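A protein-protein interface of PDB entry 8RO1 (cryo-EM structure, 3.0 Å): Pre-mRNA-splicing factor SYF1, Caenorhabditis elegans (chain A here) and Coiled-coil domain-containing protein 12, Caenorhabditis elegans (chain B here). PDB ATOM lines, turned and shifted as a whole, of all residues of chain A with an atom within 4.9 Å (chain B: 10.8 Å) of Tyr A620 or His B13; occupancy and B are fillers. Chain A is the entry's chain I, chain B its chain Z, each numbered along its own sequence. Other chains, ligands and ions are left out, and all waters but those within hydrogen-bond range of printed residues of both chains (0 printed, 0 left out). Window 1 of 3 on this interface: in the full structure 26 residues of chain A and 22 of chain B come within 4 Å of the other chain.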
ATOM      1  N   LEU A 601       2.127  10.002 -21.592  1.00  0.00           N
ATOM      2  CA  LEU A 601       3.478   9.459 -21.461  1.00  0.00           C
ATOM      3  C   LEU A 601       3.489   7.955 -21.246  1.00  0.00           C
ATOM      4  O   LEU A 601       4.416   7.280 -21.701  1.00  0.00           O
ATOM      5  CB  LEU A 601       4.234  10.133 -20.314  1.00  0.00           C
ATOM      6  CG  LEU A 601       4.604  11.615 -20.427  1.00  0.00           C
ATOM      7  CD1 LEU A 601       5.415  12.045 -19.212  1.00  0.00           C
ATOM      8  CD2 LEU A 601       5.377  11.896 -21.707  1.00  0.00           C
ATOM      9  N   ALA A 604       2.834   6.491 -24.622  1.00  0.00           N
ATOM     10  CA  ALA A 604       4.067   6.500 -25.395  1.00  0.00           C
ATOM     11  C   ALA A 604       5.007   5.390 -24.950  1.00  0.00           C
ATOM     12  O   ALA A 604       5.670   4.766 -25.783  1.00  0.00           O
ATOM     13  CB  ALA A 604       4.756   7.857 -25.258  1.00  0.00           C
ATOM     14  N   LYS A 605       5.058   5.104 -23.649  1.00  0.00           N
ATOM     15  CA  LYS A 605       5.883   3.999 -23.176  1.00  0.00           C
ATOM     16  C   LYS A 605       5.416   2.663 -23.733  1.00  0.00           C
ATOM     17  O   LYS A 605       6.237   1.845 -24.163  1.00  0.00           O
ATOM     18  CB  LYS A 605       5.850   3.952 -21.650  1.00  0.00           C
ATOM     19  CG  LYS A 605       6.704   2.855 -21.038  1.00  0.00           C
ATOM     20  CD  LYS A 605       6.785   2.956 -19.536  1.00  0.00           C
ATOM     21  CE  LYS A 605       7.720   1.897 -18.996  1.00  0.00           C
ATOM     22  NZ  LYS A 605       7.870   1.976 -17.526  1.00  0.00           N
ATOM     23  N   GLU A 608       6.222   2.678 -27.519  1.00  0.00           N
ATOM     24  CA  GLU A 608       7.657   2.533 -27.745  1.00  0.00           C
ATOM     25  C   GLU A 608       8.103   1.088 -27.575  1.00  0.00           C
ATOM     26  O   GLU A 608       8.650   0.483 -28.502  1.00  0.00           O
ATOM     27  CB  GLU A 608       8.439   3.446 -26.800  1.00  0.00           C
ATOM     28  CG  GLU A 608       8.511   4.902 -27.222  1.00  0.00           C
ATOM     29  CD  GLU A 608       9.535   5.678 -26.424  1.00  0.00           C
ATOM     30  OE1 GLU A 608       9.202   6.129 -25.308  1.00  0.00           O
ATOM     31  OE2 GLU A 608      10.672   5.838 -26.908  1.00  0.00           O
ATOM     32  N   ALA A 616       4.556   5.792 -31.626  1.00  0.00           N
ATOM     33  CA  ALA A 616       5.016   6.417 -30.388  1.00  0.00           C
ATOM     34  C   ALA A 616       5.345   7.896 -30.568  1.00  0.00           C
ATOM     35  O   ALA A 616       4.965   8.729 -29.741  1.00  0.00           O
ATOM     36  CB  ALA A 616       6.238   5.670 -29.860  1.00  0.00           C
ATOM     37  N   LEU A 617       6.050   8.244 -31.642  1.00  0.00           N
ATOM     38  CA  LEU A 617       6.332   9.651 -31.922  1.00  0.00           C
ATOM     39  C   LEU A 617       5.070  10.459 -32.190  1.00  0.00           C
ATOM     40  O   LEU A 617       4.976  11.621 -31.783  1.00  0.00           O
ATOM     41  CB  LEU A 617       7.277   9.753 -33.114  1.00  0.00           C
ATOM     42  CG  LEU A 617       8.683   9.180 -32.935  1.00  0.00           C
ATOM     43  CD1 LEU A 617       9.454   9.357 -34.221  1.00  0.00           C
ATOM     44  CD2 LEU A 617       9.421   9.831 -31.779  1.00  0.00           C
ATOM     45  N   SER A 618       4.087   9.866 -32.863  1.00  0.00           N
ATOM     46  CA  SER A 618       2.837  10.573 -33.126  1.00  0.00           C
ATOM     47  C   SER A 618       2.094  10.918 -31.846  1.00  0.00           C
ATOM     48  O   SER A 618       1.369  11.916 -31.801  1.00  0.00           O
ATOM     49  CB  SER A 618       1.942   9.737 -34.036  1.00  0.00           C
ATOM     50  OG  SER A 618       1.283   8.715 -33.310  1.00  0.00           O
ATOM     51  N   ILE A 619       2.241  10.102 -30.808  1.00  0.00           N
ATOM     52  CA  ILE A 619       1.621  10.404 -29.524  1.00  0.00           C
ATOM     53  C   ILE A 619       2.226  11.660 -28.905  1.00  0.00           C
ATOM     54  O   ILE A 619       1.518  12.464 -28.289  1.00  0.00           O
ATOM     55  CB  ILE A 619       1.763   9.175 -28.608  1.00  0.00           C
ATOM     56  CG1 ILE A 619       0.824   8.065 -29.093  1.00  0.00           C
ATOM     57  CG2 ILE A 619       1.452   9.518 -27.153  1.00  0.00           C
ATOM     58  CD1 ILE A 619       1.202   6.675 -28.633  1.00  0.00           C
ATOM     59  N   TYR A 620       3.531  11.859 -29.060  1.00  0.00           N
ATOM     60  CA  TYR A 620       4.132  13.111 -28.615  1.00  0.00           C
ATOM     61  C   TYR A 620       3.627  14.307 -29.410  1.00  0.00           C
ATOM     62  O   TYR A 620       3.404  15.379 -28.841  1.00  0.00           O
ATOM     63  CB  TYR A 620       5.651  13.032 -28.719  1.00  0.00           C
ATOM     64  CG  TYR A 620       6.289  11.919 -27.930  1.00  0.00           C
ATOM     65  CD1 TYR A 620       5.960  11.706 -26.611  1.00  0.00           C
ATOM     66  CD2 TYR A 620       7.252  11.109 -28.497  1.00  0.00           C
ATOM     67  CE1 TYR A 620       6.551  10.718 -25.886  1.00  0.00           C
ATOM     68  CE2 TYR A 620       7.845  10.113 -27.774  1.00  0.00           C
ATOM     69  CZ  TYR A 620       7.482   9.914 -26.469  1.00  0.00           C
ATOM     70  OH  TYR A 620       8.069   8.918 -25.728  1.00  0.00           O
ATOM     71  N   ASN A 621       3.431  14.147 -30.718  1.00  0.00           N
ATOM     72  CA  ASN A 621       2.825  15.216 -31.504  1.00  0.00           C
ATOM     73  C   ASN A 621       1.426  15.523 -31.003  1.00  0.00           C
ATOM     74  O   ASN A 621       0.998  16.681 -30.998  1.00  0.00           O
ATOM     75  CB  ASN A 621       2.799  14.838 -32.979  1.00  0.00           C
ATOM     76  CG  ASN A 621       2.258  15.946 -33.851  1.00  0.00           C
ATOM     77  OD1 ASN A 621       2.847  17.022 -33.938  1.00  0.00           O
ATOM     78  ND2 ASN A 621       1.135  15.690 -34.514  1.00  0.00           N
ATOM     79  N   ARG A 622       0.698  14.490 -30.588  1.00  0.00           N
ATOM     80  CA  ARG A 622      -0.608  14.674 -29.973  1.00  0.00           C
ATOM     81  C   ARG A 622      -0.487  15.225 -28.563  1.00  0.00           C
ATOM     82  O   ARG A 622      -1.342  15.996 -28.117  1.00  0.00           O
ATOM     83  CB  ARG A 622      -1.351  13.342 -29.923  1.00  0.00           C
ATOM     84  CG  ARG A 622      -1.787  12.785 -31.260  1.00  0.00           C
ATOM     85  CD  ARG A 622      -2.368  11.390 -31.100  1.00  0.00           C
ATOM     86  NE  ARG A 622      -3.583  11.396 -30.292  1.00  0.00           N
ATOM     87  CZ  ARG A 622      -4.070  10.355 -29.627  1.00  0.00           C
ATOM     88  NH1 ARG A 622      -5.171  10.510 -28.904  1.00  0.00           N
ATOM     89  NH2 ARG A 622      -3.510   9.156 -29.692  1.00  0.00           N
ATOM     90  N   ALA A 623       0.560  14.831 -27.843  1.00  0.00           N
ATOM     91  CA  ALA A 623       0.714  15.255 -26.456  1.00  0.00           C
ATOM     92  C   ALA A 623       0.904  16.760 -26.313  1.00  0.00           C
ATOM     93  O   ALA A 623       0.248  17.397 -25.484  1.00  0.00           O
ATOM     94  CB  ALA A 623       1.895  14.520 -25.825  1.00  0.00           C
ATOM     95  N   CYS A 624       1.768  17.361 -27.126  1.00  0.00           N
ATOM     96  CA  CYS A 624       1.987  18.793 -26.982  1.00  0.00           C
ATOM     97  C   CYS A 624       0.790  19.632 -27.401  1.00  0.00           C
ATOM     98  O   CYS A 624       0.684  20.784 -26.976  1.00  0.00           O
ATOM     99  CB  CYS A 624       3.197  19.202 -27.807  1.00  0.00           C
ATOM    100  SG  CYS A 624       2.996  18.894 -29.567  1.00  0.00           S
ATOM    101  N   ILE A 638      10.577  16.281 -24.617  1.00  0.00           N
ATOM    102  CA  ILE A 638      10.593  14.832 -24.828  1.00  0.00           C
ATOM    103  C   ILE A 638      10.593  14.498 -26.314  1.00  0.00           C
ATOM    104  O   ILE A 638      11.379  13.664 -26.774  1.00  0.00           O
ATOM    105  CB  ILE A 638       9.401  14.175 -24.095  1.00  0.00           C
ATOM    106  CG1 ILE A 638       9.661  14.183 -22.585  1.00  0.00           C
ATOM    107  CG2 ILE A 638       9.085  12.721 -24.629  1.00  0.00           C
ATOM    108  CD1 ILE A 638       8.555  13.605 -21.715  1.00  0.00           C
ATOM    109  N   TYR A 639       9.706  15.134 -27.081  1.00  0.00           N
ATOM    110  CA  TYR A 639       9.623  14.872 -28.515  1.00  0.00           C
ATOM    111  C   TYR A 639      10.930  15.191 -29.218  1.00  0.00           C
ATOM    112  O   TYR A 639      11.370  14.452 -30.104  1.00  0.00           O
ATOM    113  CB  TYR A 639       8.479  15.693 -29.116  1.00  0.00           C
ATOM    114  CG  TYR A 639       7.959  15.294 -30.490  1.00  0.00           C
ATOM    115  CD1 TYR A 639       8.376  14.142 -31.137  1.00  0.00           C
ATOM    116  CD2 TYR A 639       7.023  16.084 -31.129  1.00  0.00           C
ATOM    117  CE1 TYR A 639       7.882  13.801 -32.369  1.00  0.00           C
ATOM    118  CE2 TYR A 639       6.530  15.748 -32.363  1.00  0.00           C
ATOM    119  CZ  TYR A 639       6.964  14.609 -32.980  1.00  0.00           C
ATOM    120  OH  TYR A 639       6.470  14.274 -34.218  1.00  0.00           O
ATOM    121  N   LYS A 642      13.424  12.371 -28.289  1.00  0.00           N
ATOM    122  CA  LYS A 642      13.161  11.045 -28.841  1.00  0.00           C
ATOM    123  C   LYS A 642      13.295  10.971 -30.357  1.00  0.00           C
ATOM    124  O   LYS A 642      13.728   9.938 -30.874  1.00  0.00           O
ATOM    125  CB  LYS A 642      11.765  10.581 -28.425  1.00  0.00           C
ATOM    126  CG  LYS A 642      11.631  10.182 -26.957  1.00  0.00           C
ATOM    127  CD  LYS A 642      12.248   8.819 -26.682  1.00  0.00           C
ATOM    128  CE  LYS A 642      12.245   8.482 -25.206  1.00  0.00           C
ATOM    129  NZ  LYS A 642      12.844   7.149 -24.944  1.00  0.00           N
ATOM    130  N   VAL B   6       0.781   5.880 -11.510  1.00  0.00           N
ATOM    131  CA  VAL B   6       1.020   6.166 -12.927  1.00  0.00           C
ATOM    132  C   VAL B   6       2.417   6.748 -13.132  1.00  0.00           C
ATOM    133  O   VAL B   6       3.116   6.404 -14.091  1.00  0.00           O
ATOM    134  CB  VAL B   6      -0.078   7.084 -13.501  1.00  0.00           C
ATOM    135  CG1 VAL B   6      -0.081   8.469 -12.835  1.00  0.00           C
ATOM    136  CG2 VAL B   6       0.043   7.197 -15.017  1.00  0.00           C
ATOM    137  N   GLN B   7       2.838   7.643 -12.234  1.00  0.00           N
ATOM    138  CA  GLN B   7       4.179   8.226 -12.292  1.00  0.00           C
ATOM    139  C   GLN B   7       5.283   7.180 -12.178  1.00  0.00           C
ATOM    140  O   GLN B   7       6.366   7.369 -12.742  1.00  0.00           O
ATOM    141  CB  GLN B   7       4.345   9.285 -11.198  1.00  0.00           C
ATOM    142  CG  GLN B   7       3.283  10.384 -11.212  1.00  0.00           C
ATOM    143  CD  GLN B   7       3.511  11.433 -10.143  1.00  0.00           C
ATOM    144  OE1 GLN B   7       4.542  11.434  -9.469  1.00  0.00           O
ATOM    145  NE2 GLN B   7       2.546  12.335  -9.979  1.00  0.00           N
ATOM    146  N   ARG B   8       5.049   6.083 -11.455  1.00  0.00           N
ATOM    147  CA  ARG B   8       6.118   5.106 -11.256  1.00  0.00           C
ATOM    148  C   ARG B   8       6.461   4.358 -12.533  1.00  0.00           C
ATOM    149  O   ARG B   8       7.626   4.000 -12.738  1.00  0.00           O
ATOM    150  CB  ARG B   8       5.733   4.095 -10.172  1.00  0.00           C
ATOM    151  CG  ARG B   8       5.404   4.659  -8.800  1.00  0.00           C
ATOM    152  CD  ARG B   8       6.618   5.378  -8.222  1.00  0.00           C
ATOM    153  NE  ARG B   8       6.427   5.801  -6.839  1.00  0.00           N
ATOM    154  CZ  ARG B   8       5.787   6.894  -6.444  1.00  0.00           C
ATOM    155  NH1 ARG B   8       5.578   7.084  -5.145  1.00  0.00           N
ATOM    156  NH2 ARG B   8       5.406   7.833  -7.299  1.00  0.00           N
ATOM    157  N   GLU B   9       5.482   4.104 -13.396  1.00  0.00           N
ATOM    158  CA  GLU B   9       5.791   3.469 -14.671  1.00  0.00           C
ATOM    159  C   GLU B   9       6.584   4.400 -15.585  1.00  0.00           C
ATOM    160  O   GLU B   9       7.567   3.977 -16.204  1.00  0.00           O
ATOM    161  CB  GLU B   9       4.490   3.024 -15.342  1.00  0.00           C
ATOM    162  CG  GLU B   9       3.827   1.778 -14.735  1.00  0.00           C
ATOM    163  CD  GLU B   9       4.714   0.547 -14.713  1.00  0.00           C
ATOM    164  OE1 GLU B   9       5.589   0.426 -15.595  1.00  0.00           O
ATOM    165  OE2 GLU B   9       4.542  -0.293 -13.807  1.00  0.00           O
ATOM    166  N   ILE B  10       6.186   5.670 -15.672  1.00  0.00           N
ATOM    167  CA  ILE B  10       6.780   6.627 -16.608  1.00  0.00           C
ATOM    168  C   ILE B  10       8.008   7.335 -16.037  1.00  0.00           C
ATOM    169  O   ILE B  10       8.403   8.393 -16.537  1.00  0.00           O
ATOM    170  CB  ILE B  10       5.720   7.641 -17.091  1.00  0.00           C
ATOM    171  CG1 ILE B  10       5.185   8.549 -15.964  1.00  0.00           C
ATOM    172  CG2 ILE B  10       4.569   6.916 -17.780  1.00  0.00           C
ATOM    173  CD1 ILE B  10       4.594   9.835 -16.480  1.00  0.00           C
ATOM    174  N   THR B  11       8.605   6.773 -14.984  1.00  0.00           N
ATOM    175  CA  THR B  11       9.729   7.424 -14.313  1.00  0.00           C
ATOM    176  C   THR B  11      10.921   7.625 -15.244  1.00  0.00           C
ATOM    177  O   THR B  11      11.628   8.633 -15.142  1.00  0.00           O
ATOM    178  CB  THR B  11      10.120   6.601 -13.076  1.00  0.00           C
ATOM    179  OG1 THR B  11       9.176   6.842 -12.028  1.00  0.00           O
ATOM    180  CG2 THR B  11      11.531   6.932 -12.554  1.00  0.00           C
ATOM    181  N   GLU B  12      11.177   6.672 -16.142  1.00  0.00           N
ATOM    182  CA  GLU B  12      12.240   6.849 -17.129  1.00  0.00           C
ATOM    183  C   GLU B  12      12.009   8.063 -18.025  1.00  0.00           C
ATOM    184  O   GLU B  12      12.942   8.824 -18.299  1.00  0.00           O
ATOM    185  CB  GLU B  12      12.365   5.587 -17.986  1.00  0.00           C
ATOM    186  CG  GLU B  12      13.083   4.407 -17.320  1.00  0.00           C
ATOM    187  CD  GLU B  12      12.308   3.789 -16.166  1.00  0.00           C
ATOM    188  OE1 GLU B  12      11.059   3.856 -16.176  1.00  0.00           O
ATOM    189  OE2 GLU B  12      12.949   3.232 -15.250  1.00  0.00           O
ATOM    190  N   HIS B  13      10.777   8.260 -18.494  1.00  0.00           N
ATOM    191  CA  HIS B  13      10.447   9.468 -19.250  1.00  0.00           C
ATOM    192  C   HIS B  13      10.578  10.726 -18.401  1.00  0.00           C
ATOM    193  O   HIS B  13      11.150  11.729 -18.843  1.00  0.00           O
ATOM    194  CB  HIS B  13       9.055   9.345 -19.863  1.00  0.00           C
ATOM    195  CG  HIS B  13       8.912   8.159 -20.764  1.00  0.00           C
ATOM    196  ND1 HIS B  13       8.779   6.872 -20.291  1.00  0.00           N
ATOM    197  CD2 HIS B  13       8.899   8.067 -22.114  1.00  0.00           C
ATOM    198  CE1 HIS B  13       8.690   6.040 -21.313  1.00  0.00           C
ATOM    199  NE2 HIS B  13       8.755   6.740 -22.430  1.00  0.00           N
ATOM    200  N   LEU B  14      10.053  10.693 -17.179  1.00  0.00           N
ATOM    201  CA  LEU B  14      10.099  11.876 -16.329  1.00  0.00           C
ATOM    202  C   LEU B  14      11.522  12.237 -15.916  1.00  0.00           C
ATOM    203  O   LEU B  14      11.808  13.415 -15.681  1.00  0.00           O
ATOM    204  CB  LEU B  14       9.242  11.659 -15.083  1.00  0.00           C
ATOM    205  CG  LEU B  14       7.735  11.462 -15.267  1.00  0.00           C
ATOM    206  CD1 LEU B  14       7.091  11.206 -13.920  1.00  0.00           C
ATOM    207  CD2 LEU B  14       7.083  12.657 -15.948  1.00  0.00           C
ATOM    208  N   LYS B  15      12.425  11.259 -15.843  1.00  0.00           N
ATOM    209  CA  LYS B  15      13.776  11.509 -15.351  1.00  0.00           C
ATOM    210  C   LYS B  15      14.776  11.863 -16.448  1.00  0.00           C
ATOM    211  O   LYS B  15      15.463  12.884 -16.339  1.00  0.00           O
ATOM    212  CB  LYS B  15      14.252  10.268 -14.579  1.00  0.00           C
ATOM    213  CG  LYS B  15      15.579  10.405 -13.830  1.00  0.00           C
ATOM    214  CD  LYS B  15      16.811   9.961 -14.638  1.00  0.00           C
ATOM    215  CE  LYS B  15      18.100  10.486 -14.027  1.00  0.00           C
ATOM    216  NZ  LYS B  15      19.261  10.281 -14.935  1.00  0.00           N
ATOM    217  N   ASP B  16      14.853  11.062 -17.513  1.00  0.00           N
ATOM    218  CA  ASP B  16      15.929  11.165 -18.498  1.00  0.00           C
ATOM    219  C   ASP B  16      15.480  11.714 -19.845  1.00  0.00           C
ATOM    220  O   ASP B  16      16.329  11.924 -20.719  1.00  0.00           O
ATOM    221  CB  ASP B  16      16.569   9.781 -18.709  1.00  0.00           C
ATOM    222  CG  ASP B  16      18.044   9.850 -19.107  1.00  0.00           C
ATOM    223  OD1 ASP B  16      18.771  10.774 -18.679  1.00  0.00           O
ATOM    224  OD2 ASP B  16      18.485   8.959 -19.861  1.00  0.00           O
ATOM    225  N   VAL B  17      14.183  11.956 -20.033  1.00  0.00           N
ATOM    226  CA  VAL B  17      13.613  12.378 -21.308  1.00  0.00           C
ATOM    227  C   VAL B  17      12.902  13.720 -21.144  1.00  0.00           C
ATOM    228  O   VAL B  17      12.808  14.500 -22.098  1.00  0.00           O
ATOM    229  CB  VAL B  17      12.679  11.287 -21.864  1.00  0.00           C
ATOM    230  CG1 VAL B  17      12.374  11.525 -23.335  1.00  0.00           C
ATOM    231  CG2 VAL B  17      13.336   9.915 -21.706  1.00  0.00           C
ATOM    232  N   LEU B  18      12.414  14.013 -19.933  1.00  0.00           N
ATOM    233  CA  LEU B  18      11.699  15.257 -19.645  1.00  0.00           C
ATOM    234  C   LEU B  18      12.578  16.505 -19.715  1.00  0.00           C
ATOM    235  O   LEU B  18      12.055  17.611 -19.547  1.00  0.00           O
ATOM    236  CB  LEU B  18      11.064  15.156 -18.256  1.00  0.00           C
ATOM    237  CG  LEU B  18       9.893  16.064 -17.866  1.00  0.00           C
ATOM    238  CD1 LEU B  18       8.628  15.675 -18.597  1.00  0.00           C
ATOM    239  CD2 LEU B  18       9.667  16.027 -16.365  1.00  0.00           C
ATOM    240  N   HIS B  19      13.878  16.372 -19.960  1.00  0.00           N
ATOM    241  CA  HIS B  19      14.757  17.515 -20.136  1.00  0.00           C
ATOM    242  C   HIS B  19      15.982  17.040 -20.901  1.00  0.00           C
ATOM    243  O   HIS B  19      16.259  15.840 -20.975  1.00  0.00           O
ATOM    244  CB  HIS B  19      15.142  18.133 -18.792  1.00  0.00           C
ATOM    245  CG  HIS B  19      15.913  17.208 -17.905  1.00  0.00           C
ATOM    246  ND1 HIS B  19      17.287  17.239 -17.812  1.00  0.00           N
ATOM    247  CD2 HIS B  19      15.501  16.221 -17.075  1.00  0.00           C
ATOM    248  CE1 HIS B  19      17.689  16.312 -16.960  1.00  0.00           C
ATOM    249  NE2 HIS B  19      16.625  15.681 -16.499  1.00  0.00           N
ATOM    250  N   GLU B  20      16.709  17.995 -21.474  1.00  0.00           N
ATOM    251  CA  GLU B  20      18.031  17.730 -22.028  1.00  0.00           C
ATOM    252  C   GLU B  20      18.941  18.883 -21.642  1.00  0.00           C
ATOM    253  O   GLU B  20      18.579  20.051 -21.811  1.00  0.00           O
ATOM    254  CB  GLU B  20      17.974  17.553 -23.549  1.00  0.00           C
ATOM    255  CG  GLU B  20      19.283  17.093 -24.172  1.00  0.00           C
ATOM    256  CD  GLU B  20      19.152  16.805 -25.655  1.00  0.00           C
ATOM    257  OE1 GLU B  20      18.525  17.617 -26.368  1.00  0.00           O
ATOM    258  OE2 GLU B  20      19.674  15.764 -26.106  1.00  0.00           O
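Of chain B, only His B13 (3.8 Å) comes within 4 Å of Tyr A620.
His B13 touches just these residues of chain A: Lys A605, Glu A608 and Tyr A620.
Of chain B, only Ile B10 and Leu B14 come within 4 Å of Leu A601.
Ala A604 touches none of the printed residues of chain B.
Of chain B, only Glu B9, Glu B12 and His B13 come within 4 Å of Lys A605.
No residue of chain B comes within 4 Å of Ala A616.
No residue of chain B comes within 4 Å of Ser A618.
No residue of chain B comes within 4 Å of Ile A619.
No residue of chain B comes within 4 Å of Ala A623.
No residue of chain B comes within 4 Å of Cys A624.
No residue of chain B comes within 4 Å of Tyr A639.
Lys A642 touches one residue of chain B.
Printed residues of chain A within 4 Å of Leu B14: Leu A601.
Printed residues of chain B within 4 Å of Glu A608: His B13.
Of the printed residues of chain A, Leu B18 touches Ile A638.
Of the printed residues of chain B, Ile A638 touches Val B17 and Leu B18.
Arg A622 touches none of the printed residues of chain B.
His B19 touches none of the printed residues of chain A.
The nearest printed residue of chain A that does not touch Leu B18 is Leu A601 (4.9 Å).
OE1 of Glu B12 lies within salt-bridge range of NZ of Lys A605 (3.9 Å).
A ring nitrogen (NE2) of His B13 lies within hydrogen-bond range of the side-chain carboxylate (OE1) of Glu A608, at 3.0 Å.
The side-chain carboxylate of Glu B9 is in salt-bridge range of the side-chain amino group of Lys A605 (3.4 Å).
Of the 16 printed residues of chain A, 6 touch a printed residue of chain B.
Hydrophobic or aromatic side chains of chain A within 4 Å of the printed part of chain B: Leu A601, Tyr A620 and Ile A638.
Among the printed residues, 10 pairs touch across the chains.
Among the printed residues, Asp or Glu carboxylates within 4 Å of a Lys or Arg side-chain nitrogen of the other chain: Lys A605 with Glu B9 and Lys A605 with Glu B12.
The backbone carbonyl oxygen (O) of His B13 lies within hydrogen-bond range of the backbone NH (N) of Leu B18 (2.8 Å).
The side-chain hydroxyl of Tyr A620 is in hydrogen-bond range of the side-chain carboxylate of Glu A608.
The backbone carbonyl oxygen (O) of Tyr A620 lies within hydrogen-bond range of the side-chain sulfur (SG) of Cys A624 (3.6 Å).
OE2 of Glu A608 lies within salt-bridge range of NZ of Lys A642, at 3.2 Å.
Ile B10 touches Leu A601.
CD1 of Leu A601 touches CD2 of Leu B14, at 3.7 Å.
Lys A605 touches His B13.
CD2 of His B13 touches OH of Tyr A620, at 3.8 Å.
Val B17 touches Ile A638 (O to CG1, 3.2 Å).
Ile A638 touches Leu B18.
Lys A642 touches Val B17 (CE to CG1, 3.6 Å).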
